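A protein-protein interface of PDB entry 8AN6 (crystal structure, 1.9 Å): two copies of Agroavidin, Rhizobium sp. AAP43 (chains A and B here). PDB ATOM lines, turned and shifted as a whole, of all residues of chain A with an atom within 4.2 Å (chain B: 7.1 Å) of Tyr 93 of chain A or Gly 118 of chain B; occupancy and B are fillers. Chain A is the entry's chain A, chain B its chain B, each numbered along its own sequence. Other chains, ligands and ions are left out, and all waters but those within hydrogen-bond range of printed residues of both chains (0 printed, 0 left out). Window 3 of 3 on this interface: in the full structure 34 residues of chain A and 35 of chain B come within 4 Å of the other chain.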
ATOM      1  N   SER A  69      19.368   0.857  25.273  1.00  0.00           N
ATOM      2  CA  SER A  69      18.870   2.123  24.681  1.00  0.00           C
ATOM      3  C   SER A  69      18.544   3.167  25.763  1.00  0.00           C
ATOM      4  O   SER A  69      17.915   4.183  25.407  1.00  0.00           O
ATOM      5  CB  SER A  69      17.662   1.847  23.843  1.00  0.00           C
ATOM      6  OG  SER A  69      18.014   1.126  22.684  1.00  0.00           O
ATOM      7  N   GLY A  92      17.128   9.090  30.152  1.00  0.00           N
ATOM      8  CA  GLY A  92      17.074   9.338  28.700  1.00  0.00           C
ATOM      9  C   GLY A  92      17.135   8.070  27.891  1.00  0.00           C
ATOM     10  O   GLY A  92      17.510   7.005  28.436  1.00  0.00           O
ATOM     11  N   TYR A  93      16.779   8.183  26.618  1.00  0.00           N
ATOM     12  CA  TYR A  93      16.884   7.072  25.648  1.00  0.00           C
ATOM     13  C   TYR A  93      17.682   7.523  24.428  1.00  0.00           C
ATOM     14  O   TYR A  93      17.653   8.709  24.021  1.00  0.00           O
ATOM     15  CB  TYR A  93      15.504   6.555  25.263  1.00  0.00           C
ATOM     16  CG  TYR A  93      14.656   7.554  24.529  1.00  0.00           C
ATOM     17  CD1 TYR A  93      14.801   7.760  23.162  1.00  0.00           C
ATOM     18  CD2 TYR A  93      13.676   8.266  25.201  1.00  0.00           C
ATOM     19  CE1 TYR A  93      14.016   8.682  22.485  1.00  0.00           C
ATOM     20  CE2 TYR A  93      12.871   9.176  24.537  1.00  0.00           C
ATOM     21  CZ  TYR A  93      13.039   9.380  23.178  1.00  0.00           C
ATOM     22  OH  TYR A  93      12.244  10.287  22.549  1.00  0.00           O
ATOM     23  N   ALA A  94      18.394   6.551  23.870  1.00  0.00           N
ATOM     24  CA  ALA A  94      19.132   6.648  22.602  1.00  0.00           C
ATOM     25  C   ALA A  94      18.119   6.869  21.477  1.00  0.00           C
ATOM     26  O   ALA A  94      17.165   6.064  21.368  1.00  0.00           O
ATOM     27  CB  ALA A  94      19.908   5.381  22.398  1.00  0.00           C
ATOM     28  N   ARG A  95      18.281   7.956  20.728  1.00  0.00           N
ATOM     29  CA  ARG A  95      17.593   8.171  19.430  1.00  0.00           C
ATOM     30  C   ARG A  95      18.660   8.138  18.331  1.00  0.00           C
ATOM     31  O   ARG A  95      19.555   8.998  18.334  1.00  0.00           O
ATOM     32  CB  ARG A  95      16.790   9.473  19.436  1.00  0.00           C
ATOM     33  CG  ARG A  95      15.661   9.507  18.416  1.00  0.00           C
ATOM     34  CD  ARG A  95      14.799  10.748  18.528  1.00  0.00           C
ATOM     35  NE  ARG A  95      15.655  11.933  18.563  1.00  0.00           N
ATOM     36  CZ  ARG A  95      15.250  13.167  18.864  1.00  0.00           C
ATOM     37  NH1 ARG A  95      16.116  14.171  18.848  1.00  0.00           N
ATOM     38  NH2 ARG A  95      13.984  13.392  19.161  1.00  0.00           N
ATOM     39  N   GLN A 103      21.793  10.478  19.617  1.00  0.00           N
ATOM     40  CA  GLN A 103      21.455  11.530  20.612  1.00  0.00           C
ATOM     41  C   GLN A 103      20.888  10.856  21.857  1.00  0.00           C
ATOM     42  O   GLN A 103      20.339   9.737  21.719  1.00  0.00           O
ATOM     43  CB  GLN A 103      20.457  12.535  20.047  1.00  0.00           C
ATOM     44  CG  GLN A 103      21.047  13.368  18.930  1.00  0.00           C
ATOM     45  CD  GLN A 103      20.071  14.367  18.355  1.00  0.00           C
ATOM     46  OE1 GLN A 103      19.027  14.006  17.823  1.00  0.00           O
ATOM     47  NE2 GLN A 103      20.430  15.634  18.423  1.00  0.00           N
ATOM     48  N   ILE A 104      20.995  11.530  23.003  1.00  0.00           N
ATOM     49  CA  ILE A 104      20.267  11.153  24.249  1.00  0.00           C
ATOM     50  C   ILE A 104      19.132  12.148  24.452  1.00  0.00           C
ATOM     51  O   ILE A 104      19.422  13.314  24.718  1.00  0.00           O
ATOM     52  CB  ILE A 104      21.200  11.093  25.476  1.00  0.00           C
ATOM     53  CG1 ILE A 104      22.522  10.429  25.106  1.00  0.00           C
ATOM     54  CG2 ILE A 104      20.492  10.395  26.634  1.00  0.00           C
ATOM     55  CD1 ILE A 104      23.512  10.367  26.221  1.00  0.00           C
ATOM     56  N   VAL A 105      17.894  11.670  24.332  1.00  0.00           N
ATOM     57  CA  VAL A 105      16.670  12.455  24.633  1.00  0.00           C
ATOM     58  C   VAL A 105      16.352  12.259  26.115  1.00  0.00           C
ATOM     59  O   VAL A 105      16.085  11.103  26.512  1.00  0.00           O
ATOM     60  CB  VAL A 105      15.510  12.031  23.723  1.00  0.00           C
ATOM     61  CG1 VAL A 105      14.292  12.911  23.927  1.00  0.00           C
ATOM     62  CG2 VAL A 105      15.937  12.030  22.263  1.00  0.00           C
ATOM     63  N   ALA B 111      12.842   6.662  31.597  1.00  0.00           N
ATOM     64  CA  ALA B 111      13.015   6.520  30.138  1.00  0.00           C
ATOM     65  C   ALA B 111      12.950   5.031  29.806  1.00  0.00           C
ATOM     66  O   ALA B 111      13.499   4.228  30.587  1.00  0.00           O
ATOM     67  CB  ALA B 111      14.328   7.090  29.690  1.00  0.00           C
ATOM     68  N   PHE B 112      12.286   4.698  28.700  1.00  0.00           N
ATOM     69  CA  PHE B 112      12.128   3.319  28.181  1.00  0.00           C
ATOM     70  C   PHE B 112      11.859   3.362  26.680  1.00  0.00           C
ATOM     71  O   PHE B 112      11.366   4.384  26.179  1.00  0.00           O
ATOM     72  CB  PHE B 112      10.997   2.590  28.899  1.00  0.00           C
ATOM     73  CG  PHE B 112       9.616   3.133  28.638  1.00  0.00           C
ATOM     74  CD1 PHE B 112       9.118   4.195  29.371  1.00  0.00           C
ATOM     75  CD2 PHE B 112       8.804   2.554  27.677  1.00  0.00           C
ATOM     76  CE1 PHE B 112       7.832   4.662  29.152  1.00  0.00           C
ATOM     77  CE2 PHE B 112       7.523   3.030  27.453  1.00  0.00           C
ATOM     78  CZ  PHE B 112       7.033   4.075  28.201  1.00  0.00           C
ATOM     79  N   VAL B 113      12.198   2.264  26.010  1.00  0.00           N
ATOM     80  CA  VAL B 113      11.860   1.986  24.589  1.00  0.00           C
ATOM     81  C   VAL B 113      10.674   1.022  24.582  1.00  0.00           C
ATOM     82  O   VAL B 113      10.860  -0.132  24.985  1.00  0.00           O
ATOM     83  CB  VAL B 113      13.076   1.402  23.848  1.00  0.00           C
ATOM     84  CG1 VAL B 113      12.821   1.293  22.347  1.00  0.00           C
ATOM     85  CG2 VAL B 113      14.329   2.219  24.127  1.00  0.00           C
ATOM     86  N   GLY B 114       9.496   1.504  24.183  1.00  0.00           N
ATOM     87  CA  GLY B 114       8.281   0.682  24.019  1.00  0.00           C
ATOM     88  C   GLY B 114       8.095   0.255  22.572  1.00  0.00           C
ATOM     89  O   GLY B 114       9.085   0.291  21.802  1.00  0.00           O
ATOM     90  N   LYS B 115       6.871  -0.132  22.207  1.00  0.00           N
ATOM     91  CA  LYS B 115       6.494  -0.475  20.810  1.00  0.00           C
ATOM     92  C   LYS B 115       6.638   0.789  19.954  1.00  0.00           C
ATOM     93  O   LYS B 115       7.288   0.716  18.892  1.00  0.00           O
ATOM     94  CB  LYS B 115       5.086  -1.078  20.775  1.00  0.00           C
ATOM     95  CG  LYS B 115       4.888  -2.268  21.708  1.00  0.00           C
ATOM     96  CD  LYS B 115       4.494  -3.549  21.006  1.00  0.00           C
ATOM     97  CE  LYS B 115       5.106  -4.782  21.641  1.00  0.00           C
ATOM     98  NZ  LYS B 115       4.929  -5.979  20.784  1.00  0.00           N
ATOM     99  N   ALA B 116       6.125   1.919  20.450  1.00  0.00           N
ATOM    100  CA  ALA B 116       6.215   3.254  19.808  1.00  0.00           C
ATOM    101  C   ALA B 116       7.604   3.874  20.033  1.00  0.00           C
ATOM    102  O   ALA B 116       7.752   5.080  19.760  1.00  0.00           O
ATOM    103  CB  ALA B 116       5.117   4.143  20.342  1.00  0.00           C
ATOM    104  N   GLY B 117       8.586   3.088  20.491  1.00  0.00           N
ATOM    105  CA  GLY B 117       9.973   3.541  20.730  1.00  0.00           C
ATOM    106  C   GLY B 117      10.104   4.403  21.982  1.00  0.00           C
ATOM    107  O   GLY B 117       9.209   4.334  22.867  1.00  0.00           O
ATOM    108  N   GLY B 118      11.182   5.193  22.040  1.00  0.00           N
ATOM    109  CA  GLY B 118      11.587   6.054  23.172  1.00  0.00           C
ATOM    110  C   GLY B 118      10.434   6.826  23.787  1.00  0.00           C
ATOM    111  O   GLY B 118       9.735   7.521  23.062  1.00  0.00           O
ATOM    112  N   LYS B 119      10.246   6.700  25.096  1.00  0.00           N
ATOM    113  CA  LYS B 119       9.284   7.505  25.897  1.00  0.00           C
ATOM    114  C   LYS B 119       9.918   7.831  27.254  1.00  0.00           C
ATOM    115  O   LYS B 119      10.872   7.134  27.655  1.00  0.00           O
ATOM    116  CB  LYS B 119       7.974   6.735  26.110  1.00  0.00           C
ATOM    117  CG  LYS B 119       7.065   6.609  24.890  1.00  0.00           C
ATOM    118  CD  LYS B 119       6.317   7.885  24.557  1.00  0.00           C
ATOM    119  CE  LYS B 119       5.233   7.707  23.509  1.00  0.00           C
ATOM    120  NZ  LYS B 119       5.800   7.364  22.179  1.00  0.00           N
ATOM    121  N   ILE B 120       9.382   8.840  27.937  1.00  0.00           N
ATOM    122  CA  ILE B 120       9.788   9.249  29.309  1.00  0.00           C
ATOM    123  C   ILE B 120       8.526   9.506  30.142  1.00  0.00           C
ATOM    124  O   ILE B 120       7.670  10.298  29.715  1.00  0.00           O
ATOM    125  CB  ILE B 120      10.738  10.458  29.257  1.00  0.00           C
ATOM    126  CG1 ILE B 120      12.006  10.101  28.482  1.00  0.00           C
ATOM    127  CG2 ILE B 120      11.041  10.971  30.658  1.00  0.00           C
ATOM    128  CD1 ILE B 120      12.965  11.253  28.293  1.00  0.00           C
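Among the printed residues, merely in contact across the chains: Ser 69 of chain A with Val 113 of chain B (3.4 Å), Gly 92 of chain A with Ala 111 of chain B (3.4 Å), Tyr 93 of chain A with Gly 118 of chain B (3.5 Å), Val 105 of chain A with Ile 120 of chain B (3.6 Å) and Tyr 93 of chain A with Lys 119 of chain B (3.7 Å).
No position is printed for both chains.
Of the 5 pairs that touch across the chains among the printed residues, none has its exchanged pair printed and touching as well.
Hydrophobic or aromatic side chains of chain B within 4 Å of the printed part of chain A: Ala 111, Val 113 and Ile 120.
Printed residues of chain A that touch a printed residue of chain B: Ser 69, Gly 92, Tyr 93 and Val 105.
Hydrophobic or aromatic side chains of chain A that line the printed part of chain B: Tyr 93.
Among the printed residues, no Asp or Glu carboxylate lies within 4 Å of a Lys or Arg side-chain nitrogen of the other chain.
N of Ala 94 of chain A sits at hydrogen-bond distance from O of Ser 69 of chain A (2.9 Å).
The backbone carbonyl oxygen of Tyr 93 of chain A is in hydrogen-bond range of the backbone NH of Val 105 of chain A (3.0 Å).
N of Lys 119 of chain B sits at hydrogen-bond distance from O of Phe 112 of chain B, at 2.8 Å.
Printed residues of chain B within 4 Å of Ser 69 of chain A: Val 113.
Of the printed residues of chain B, Gly 92 of chain A touches Ala 111.
Tyr 93 of chain A touches two residues of chain B.
Printed residues of chain B within 4 Å of Val 105 of chain A: Ile 120 (3.6 Å).
Gly 117 of chain B touches none of the printed residues of chain A.
Gly 118 of chain B touches just one residue of chain A: Tyr 93.
Of the printed residues of chain A, Lys 119 of chain B touches Tyr 93 (3.7 Å).
Of the printed residues of chain A, Ile 120 of chain B touches Val 105.
The nearest residue of chain B that does not touch Tyr 93 of chain A is Ala 111 of chain B (4.1 Å).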
